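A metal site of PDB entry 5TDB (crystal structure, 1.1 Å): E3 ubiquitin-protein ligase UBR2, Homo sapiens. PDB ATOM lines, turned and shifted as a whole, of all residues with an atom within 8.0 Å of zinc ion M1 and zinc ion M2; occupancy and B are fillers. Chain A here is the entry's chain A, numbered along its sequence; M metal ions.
Zinc ion M1 is bound by the side-chain sulfur of Cys 7, the side-chain sulfur of Cys 57, the side-chain sulfur of Cys 32 and the side-chain sulfur of Cys 35.
Four residues have an atom within 4 Å of zinc ion M1: Cys 7, Cys 32, Cys 35 and Cys 57.
Of the 28 residues printed, 4 come within 4 Å of zinc ion M2.
SG of Cys 57 sits close to N of Cys 59 (3.4 Å).
The side-chain sulfur of Cys 7 lies close to the backbone NH of Arg 9, at 3.5 Å.
SG of Cys 71 lies close to N of Lys 73 (3.4 Å).
O of Arg 9 sits at hydrogen-bond distance from N of Cys 57, 2.9 Å away.
The side-chain sulfur (SG) of Cys 32 sits close to the guanidinium group (NE) of Arg 9, 3.5 Å away.
SG of Cys 32 lies close to N of Glu 34, at 3.7 Å.
Zinc ion M2 is bound by ND1 of His 74 (2.1 Å), SG of Cys 59 (2.3 Å), SG of Cys 71 (2.3 Å) and SG of Cys 35 (2.4 Å).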
ATOM      1  N   LEU A   6      24.213   9.218 -15.227  1.00  0.00           N
ATOM      2  CA  LEU A   6      22.772   9.009 -15.414  1.00  0.00           C
ATOM      3  C   LEU A   6      21.917   9.716 -14.353  1.00  0.00           C
ATOM      4  O   LEU A   6      20.676   9.619 -14.397  1.00  0.00           O
ATOM      5  CB  LEU A   6      22.455   7.504 -15.467  1.00  0.00           C
ATOM      6  N   CYS A   7      22.550  10.394 -13.392  1.00  0.00           N
ATOM      7  CA  CYS A   7      21.818  11.272 -12.479  1.00  0.00           C
ATOM      8  C   CYS A   7      21.374  12.532 -13.213  1.00  0.00           C
ATOM      9  O   CYS A   7      20.184  12.704 -13.482  1.00  0.00           O
ATOM     10  CB  CYS A   7      22.666  11.636 -11.261  1.00  0.00           C
ATOM     11  SG  CYS A   7      21.725  12.708 -10.181  1.00  0.00           S
ATOM     12  N   GLY A   8      22.319  13.413 -13.537  1.00  0.00           N
ATOM     13  CA  GLY A   8      22.032  14.658 -14.236  1.00  0.00           C
ATOM     14  C   GLY A   8      21.204  15.677 -13.468  1.00  0.00           C
ATOM     15  O   GLY A   8      20.813  16.681 -14.073  1.00  0.00           O
ATOM     16  N   ARG A   9      20.961  15.478 -12.173  1.00  0.00           N
ATOM     17  CA  ARG A   9      20.041  16.343 -11.429  1.00  0.00           C
ATOM     18  C   ARG A   9      20.440  17.801 -11.554  1.00  0.00           C
ATOM     19  O   ARG A   9      21.583  18.164 -11.296  1.00  0.00           O
ATOM     20  CB  ARG A   9      20.043  15.961  -9.942  1.00  0.00           C
ATOM     21  CG  ARG A   9      19.054  16.799  -9.102  1.00  0.00           C
ATOM     22  CD  ARG A   9      19.247  16.719  -7.587  1.00  0.00           C
ATOM     23  NE  ARG A   9      19.051  15.375  -7.068  1.00  0.00           N
ATOM     24  CZ  ARG A   9      18.632  15.090  -5.831  1.00  0.00           C
ATOM     25  NH1 ARG A   9      18.312  16.049  -4.967  1.00  0.00           N
ATOM     26  NH2 ARG A   9      18.489  13.833  -5.457  1.00  0.00           N
ATOM     27  N   VAL A  10      19.474  18.658 -11.908  1.00  0.00           N
ATOM     28  CA  VAL A  10      19.666  20.104 -11.917  1.00  0.00           C
ATOM     29  C   VAL A  10      19.261  20.652 -10.552  1.00  0.00           C
ATOM     30  O   VAL A  10      18.160  20.372 -10.058  1.00  0.00           O
ATOM     31  CB  VAL A  10      18.853  20.757 -13.043  1.00  0.00           C
ATOM     32  CG1 VAL A  10      18.951  22.277 -12.941  1.00  0.00           C
ATOM     33  CG2 VAL A  10      19.358  20.277 -14.378  1.00  0.00           C
ATOM     34  N   PHE A  11      20.162  21.397  -9.925  1.00  0.00           N
ATOM     35  CA  PHE A  11      19.922  21.888  -8.567  1.00  0.00           C
ATOM     36  C   PHE A  11      18.869  22.984  -8.527  1.00  0.00           C
ATOM     37  O   PHE A  11      18.795  23.854  -9.404  1.00  0.00           O
ATOM     38  CB  PHE A  11      21.214  22.382  -7.924  1.00  0.00           C
ATOM     39  CG  PHE A  11      22.248  21.321  -7.816  1.00  0.00           C
ATOM     40  CD1 PHE A  11      22.026  20.206  -7.037  1.00  0.00           C
ATOM     41  CD2 PHE A  11      23.439  21.421  -8.530  1.00  0.00           C
ATOM     42  CE1 PHE A  11      22.972  19.222  -6.939  1.00  0.00           C
ATOM     43  CE2 PHE A  11      24.389  20.429  -8.432  1.00  0.00           C
ATOM     44  CZ  PHE A  11      24.150  19.326  -7.657  1.00  0.00           C
ATOM     45  N   GLU A  15      19.283  24.318  -2.618  1.00  0.00           N
ATOM     46  CA  GLU A  15      19.558  22.891  -2.479  1.00  0.00           C
ATOM     47  C   GLU A  15      21.036  22.652  -2.151  1.00  0.00           C
ATOM     48  O   GLU A  15      21.919  23.245  -2.791  1.00  0.00           O
ATOM     49  CB  GLU A  15      19.189  22.176  -3.758  1.00  0.00           C
ATOM     50  CG  GLU A  15      19.172  20.702  -3.607  1.00  0.00           C
ATOM     51  CD  GLU A  15      18.701  19.976  -4.856  1.00  0.00           C
ATOM     52  OE1 GLU A  15      19.021  18.791  -4.952  1.00  0.00           O
ATOM     53  OE2 GLU A  15      18.038  20.541  -5.743  1.00  0.00           O
ATOM     54  N   VAL A  30      30.658  18.588  -8.375  1.00  0.00           N
ATOM     55  CA  VAL A  30      29.734  18.433  -7.259  1.00  0.00           C
ATOM     56  C   VAL A  30      28.854  17.209  -7.455  1.00  0.00           C
ATOM     57  O   VAL A  30      28.647  16.711  -8.559  1.00  0.00           O
ATOM     58  CB  VAL A  30      28.861  19.688  -7.062  1.00  0.00           C
ATOM     59  CG1 VAL A  30      29.703  20.857  -6.581  1.00  0.00           C
ATOM     60  CG2 VAL A  30      28.121  20.014  -8.350  1.00  0.00           C
ATOM     61  N   LEU A  31      28.308  16.761  -6.329  1.00  0.00           N
ATOM     62  CA  LEU A  31      27.304  15.721  -6.253  1.00  0.00           C
ATOM     63  C   LEU A  31      26.043  16.235  -5.564  1.00  0.00           C
ATOM     64  O   LEU A  31      26.112  17.044  -4.627  1.00  0.00           O
ATOM     65  CB  LEU A  31      27.828  14.517  -5.468  1.00  0.00           C
ATOM     66  CG  LEU A  31      29.031  13.811  -6.097  1.00  0.00           C
ATOM     67  CD1 LEU A  31      29.541  12.736  -5.173  1.00  0.00           C
ATOM     68  CD2 LEU A  31      28.702  13.220  -7.450  1.00  0.00           C
ATOM     69  N   CYS A  32      24.891  15.750  -6.038  1.00  0.00           N
ATOM     70  CA  CYS A  32      23.634  15.980  -5.329  1.00  0.00           C
ATOM     71  C   CYS A  32      23.621  15.166  -4.038  1.00  0.00           C
ATOM     72  O   CYS A  32      24.460  14.295  -3.803  1.00  0.00           O
ATOM     73  CB  CYS A  32      22.429  15.636  -6.210  1.00  0.00           C
ATOM     74  SG  CYS A  32      22.154  13.845  -6.474  1.00  0.00           S
ATOM     75  N   MET A  33      22.629  15.441  -3.206  1.00  0.00           N
ATOM     76  CA  MET A  33      22.558  14.777  -1.915  1.00  0.00           C
ATOM     77  C   MET A  33      22.456  13.266  -2.061  1.00  0.00           C
ATOM     78  O   MET A  33      23.089  12.512  -1.316  1.00  0.00           O
ATOM     79  CB  MET A  33      21.357  15.336  -1.153  1.00  0.00           C
ATOM     80  CG  MET A  33      21.174  14.760   0.200  1.00  0.00           C
ATOM     81  SD  MET A  33      19.639  15.350   0.928  1.00  0.00           S
ATOM     82  CE  MET A  33      19.401  13.974   2.041  1.00  0.00           C
ATOM     83  N   GLU A  34      21.607  12.800  -2.990  1.00  0.00           N
ATOM     84  CA  GLU A  34      21.430  11.361  -3.165  1.00  0.00           C
ATOM     85  C   GLU A  34      22.743  10.694  -3.540  1.00  0.00           C
ATOM     86  O   GLU A  34      23.130   9.654  -2.981  1.00  0.00           O
ATOM     87  CB  GLU A  34      20.377  11.101  -4.248  1.00  0.00           C
ATOM     88  CG  GLU A  34      20.236   9.613  -4.565  1.00  0.00           C
ATOM     89  CD  GLU A  34      19.294   9.277  -5.696  1.00  0.00           C
ATOM     90  OE1 GLU A  34      18.824  10.214  -6.388  1.00  0.00           O
ATOM     91  OE2 GLU A  34      19.056   8.068  -5.897  1.00  0.00           O
ATOM     92  N   CYS A  35      23.442  11.274  -4.506  1.00  0.00           N
ATOM     93  CA  CYS A  35      24.673  10.676  -5.004  1.00  0.00           C
ATOM     94  C   CYS A  35      25.787  10.764  -3.970  1.00  0.00           C
ATOM     95  O   CYS A  35      26.517   9.786  -3.756  1.00  0.00           O
ATOM     96  CB  CYS A  35      25.042  11.322  -6.343  1.00  0.00           C
ATOM     97  SG  CYS A  35      23.812  10.929  -7.610  1.00  0.00           S
ATOM     98  N   PHE A  36      25.898  11.905  -3.280  1.00  0.00           N
ATOM     99  CA  PHE A  36      26.903  12.058  -2.234  1.00  0.00           C
ATOM    100  C   PHE A  36      26.752  10.970  -1.167  1.00  0.00           C
ATOM    101  O   PHE A  36      27.735  10.330  -0.784  1.00  0.00           O
ATOM    102  CB  PHE A  36      26.799  13.468  -1.609  1.00  0.00           C
ATOM    103  CG  PHE A  36      27.628  13.626  -0.383  1.00  0.00           C
ATOM    104  CD1 PHE A  36      29.017  13.702  -0.457  1.00  0.00           C
ATOM    105  CD2 PHE A  36      27.029  13.710   0.875  1.00  0.00           C
ATOM    106  CE1 PHE A  36      29.774  13.854   0.700  1.00  0.00           C
ATOM    107  CE2 PHE A  36      27.784  13.850   2.006  1.00  0.00           C
ATOM    108  CZ  PHE A  36      29.153  13.914   1.909  1.00  0.00           C
ATOM    109  N   GLY A  38      25.470   8.092  -1.266  1.00  0.00           N
ATOM    110  CA  GLY A  38      25.746   6.766  -1.780  1.00  0.00           C
ATOM    111  C   GLY A  38      27.121   6.614  -2.415  1.00  0.00           C
ATOM    112  O   GLY A  38      27.358   5.633  -3.141  1.00  0.00           O
ATOM    113  N   SER A  39      28.041   7.541  -2.117  1.00  0.00           N
ATOM    114  CA  SER A  39      29.359   7.585  -2.752  1.00  0.00           C
ATOM    115  C   SER A  39      30.452   7.352  -1.707  1.00  0.00           C
ATOM    116  O   SER A  39      30.230   7.440  -0.498  1.00  0.00           O
ATOM    117  CB  SER A  39      29.609   8.947  -3.421  1.00  0.00           C
ATOM    118  OG  SER A  39      29.951   9.955  -2.477  1.00  0.00           O
ATOM    119  N   PHE A  56      24.442  21.300 -12.075  1.00  0.00           N
ATOM    120  CA  PHE A  56      23.979  19.920 -12.152  1.00  0.00           C
ATOM    121  C   PHE A  56      24.961  18.982 -11.450  1.00  0.00           C
ATOM    122  O   PHE A  56      26.154  19.270 -11.289  1.00  0.00           O
ATOM    123  CB  PHE A  56      23.704  19.474 -13.601  1.00  0.00           C
ATOM    124  CG  PHE A  56      24.918  19.551 -14.502  1.00  0.00           C
ATOM    125  CD1 PHE A  56      25.801  18.486 -14.590  1.00  0.00           C
ATOM    126  CD2 PHE A  56      25.176  20.700 -15.245  1.00  0.00           C
ATOM    127  CE1 PHE A  56      26.926  18.560 -15.385  1.00  0.00           C
ATOM    128  CE2 PHE A  56      26.285  20.776 -16.058  1.00  0.00           C
ATOM    129  CZ  PHE A  56      27.160  19.706 -16.128  1.00  0.00           C
ATOM    130  N   CYS A  57      24.442  17.813 -11.093  1.00  0.00           N
ATOM    131  CA  CYS A  57      25.225  16.775 -10.440  1.00  0.00           C
ATOM    132  C   CYS A  57      26.181  16.113 -11.431  1.00  0.00           C
ATOM    133  O   CYS A  57      25.783  15.783 -12.546  1.00  0.00           O
ATOM    134  CB  CYS A  57      24.259  15.736  -9.871  1.00  0.00           C
ATOM    135  SG  CYS A  57      25.071  14.337  -9.059  1.00  0.00           S
ATOM    136  N   ASP A  58      27.425  15.893 -10.991  1.00  0.00           N
ATOM    137  CA  ASP A  58      28.479  15.297 -11.797  1.00  0.00           C
ATOM    138  C   ASP A  58      28.674  13.805 -11.530  1.00  0.00           C
ATOM    139  O   ASP A  58      29.700  13.241 -11.934  1.00  0.00           O
ATOM    140  CB  ASP A  58      29.790  16.041 -11.591  1.00  0.00           C
ATOM    141  CG  ASP A  58      29.705  17.480 -12.012  1.00  0.00           C
ATOM    142  OD1 ASP A  58      29.333  17.748 -13.190  1.00  0.00           O
ATOM    143  OD2 ASP A  58      29.982  18.371 -11.173  1.00  0.00           O
ATOM    144  N   CYS A  59      27.714  13.147 -10.875  1.00  0.00           N
ATOM    145  CA  CYS A  59      27.816  11.716 -10.681  1.00  0.00           C
ATOM    146  C   CYS A  59      27.905  11.027 -12.035  1.00  0.00           C
ATOM    147  O   CYS A  59      27.083  11.263 -12.931  1.00  0.00           O
ATOM    148  CB  CYS A  59      26.588  11.195  -9.922  1.00  0.00           C
ATOM    149  SG  CYS A  59      26.588   9.387  -9.769  1.00  0.00           S
ATOM    150  N   GLY A  60      28.899  10.160 -12.168  1.00  0.00           N
ATOM    151  CA  GLY A  60      29.109   9.413 -13.368  1.00  0.00           C
ATOM    152  C   GLY A  60      30.066  10.034 -14.350  1.00  0.00           C
ATOM    153  O   GLY A  60      30.398   9.391 -15.355  1.00  0.00           O
ATOM    154  N   PRO A  69      33.876   8.059  -9.236  1.00  0.00           N
ATOM    155  CA  PRO A  69      32.987   8.934 -10.036  1.00  0.00           C
ATOM    156  C   PRO A  69      31.514   8.606  -9.929  1.00  0.00           C
ATOM    157  O   PRO A  69      30.686   9.494 -10.155  1.00  0.00           O
ATOM    158  CB  PRO A  69      33.513   8.752 -11.466  1.00  0.00           C
ATOM    159  CG  PRO A  69      34.127   7.411 -11.454  1.00  0.00           C
ATOM    160  CD  PRO A  69      34.768   7.259 -10.100  1.00  0.00           C
ATOM    161  N   TYR A  70      31.154   7.364  -9.619  1.00  0.00           N
ATOM    162  CA  TYR A  70      29.753   6.962  -9.543  1.00  0.00           C
ATOM    163  C   TYR A  70      29.384   6.660  -8.094  1.00  0.00           C
ATOM    164  O   TYR A  70      30.209   6.184  -7.324  1.00  0.00           O
ATOM    165  CB  TYR A  70      29.518   5.693 -10.379  1.00  0.00           C
ATOM    166  CG  TYR A  70      29.505   5.874 -11.899  1.00  0.00           C
ATOM    167  CD1 TYR A  70      30.660   5.782 -12.654  1.00  0.00           C
ATOM    168  CD2 TYR A  70      28.308   6.120 -12.570  1.00  0.00           C
ATOM    169  CE1 TYR A  70      30.640   5.925 -14.041  1.00  0.00           C
ATOM    170  CE2 TYR A  70      28.275   6.267 -13.961  1.00  0.00           C
ATOM    171  CZ  TYR A  70      29.446   6.184 -14.685  1.00  0.00           C
ATOM    172  OH  TYR A  70      29.409   6.328 -16.067  1.00  0.00           O
ATOM    173  N   CYS A  71      28.125   6.910  -7.742  1.00  0.00           N
ATOM    174  CA  CYS A  71      27.526   6.432  -6.501  1.00  0.00           C
ATOM    175  C   CYS A  71      26.937   5.027  -6.688  1.00  0.00           C
ATOM    176  O   CYS A  71      26.876   4.496  -7.789  1.00  0.00           O
ATOM    177  CB  CYS A  71      26.446   7.413  -6.051  1.00  0.00           C
ATOM    178  SG  CYS A  71      24.881   7.292  -6.951  1.00  0.00           S
ATOM    179  N   GLN A  72      26.469   4.439  -5.583  1.00  0.00           N
ATOM    180  CA  GLN A  72      25.943   3.081  -5.639  1.00  0.00           C
ATOM    181  C   GLN A  72      24.670   2.974  -6.480  1.00  0.00           C
ATOM    182  O   GLN A  72      24.378   1.905  -7.021  1.00  0.00           O
ATOM    183  CB  GLN A  72      25.621   2.587  -4.240  1.00  0.00           C
ATOM    184  CG  GLN A  72      26.804   2.346  -3.359  1.00  0.00           C
ATOM    185  CD  GLN A  72      26.426   1.637  -2.074  1.00  0.00           C
ATOM    186  OE1 GLN A  72      25.669   2.169  -1.249  1.00  0.00           O
ATOM    187  NE2 GLN A  72      26.918   0.424  -1.893  1.00  0.00           N
ATOM    188  N   LYS A  73      23.902   4.045  -6.586  1.00  0.00           N
ATOM    189  CA  LYS A  73      22.666   4.017  -7.345  1.00  0.00           C
ATOM    190  C   LYS A  73      22.901   4.084  -8.848  1.00  0.00           C
ATOM    191  O   LYS A  73      22.097   3.518  -9.610  1.00  0.00           O
ATOM    192  CB  LYS A  73      21.782   5.187  -6.881  1.00  0.00           C
ATOM    193  CG  LYS A  73      20.312   5.064  -7.230  1.00  0.00           C
ATOM    194  CD  LYS A  73      19.969   5.978  -8.367  1.00  0.00           C
ATOM    195  CE  LYS A  73      18.469   5.953  -8.670  1.00  0.00           C
ATOM    196  NZ  LYS A  73      17.625   6.632  -7.645  1.00  0.00           N
ATOM    197  N   HIS A  74      23.976   4.738  -9.304  1.00  0.00           N
ATOM    198  CA  HIS A  74      24.171   4.955 -10.730  1.00  0.00           C
ATOM    199  C   HIS A  74      25.298   4.127 -11.335  1.00  0.00           C
ATOM    200  O   HIS A  74      25.381   4.030 -12.564  1.00  0.00           O
ATOM    201  CB  HIS A  74      24.385   6.458 -11.020  1.00  0.00           C
ATOM    202  CG  HIS A  74      23.178   7.287 -10.712  1.00  0.00           C
ATOM    203  ND1 HIS A  74      23.139   8.231  -9.700  1.00  0.00           N
ATOM    204  CD2 HIS A  74      21.941   7.259 -11.256  1.00  0.00           C
ATOM    205  CE1 HIS A  74      21.917   8.730  -9.641  1.00  0.00           C
ATOM    206  NE2 HIS A  74      21.178   8.176 -10.586  1.00  0.00           N
ATOM    207  N   GLU A  75      26.118   3.466 -10.513  1.00  0.00           N
ATOM    208  CA  GLU A  75      27.206   2.639 -11.033  1.00  0.00           C
ATOM    209  C   GLU A  75      26.687   1.464 -11.853  1.00  0.00           C
ATOM    210  O   GLU A  75      27.429   0.970 -12.709  1.00  0.00           O
ATOM    211  CB  GLU A  75      28.046   2.082  -9.870  1.00  0.00           C
ATOM    212  CG  GLU A  75      27.324   1.053  -9.006  1.00  0.00           C
ATOM    213  CD  GLU A  75      28.154   0.560  -7.843  1.00  0.00           C
ATOM    214  OE1 GLU A  75      29.395   0.644  -7.938  1.00  0.00           O
ATOM    215  OE2 GLU A  75      27.564   0.087  -6.834  1.00  0.00           O
HETATM  216 ZN    ZN M   1      23.200  13.091  -8.431  1.00  0.00          ZN
HETATM  217 ZN    ZN M   2      24.706   8.961  -8.554  1.00  0.00          ZN
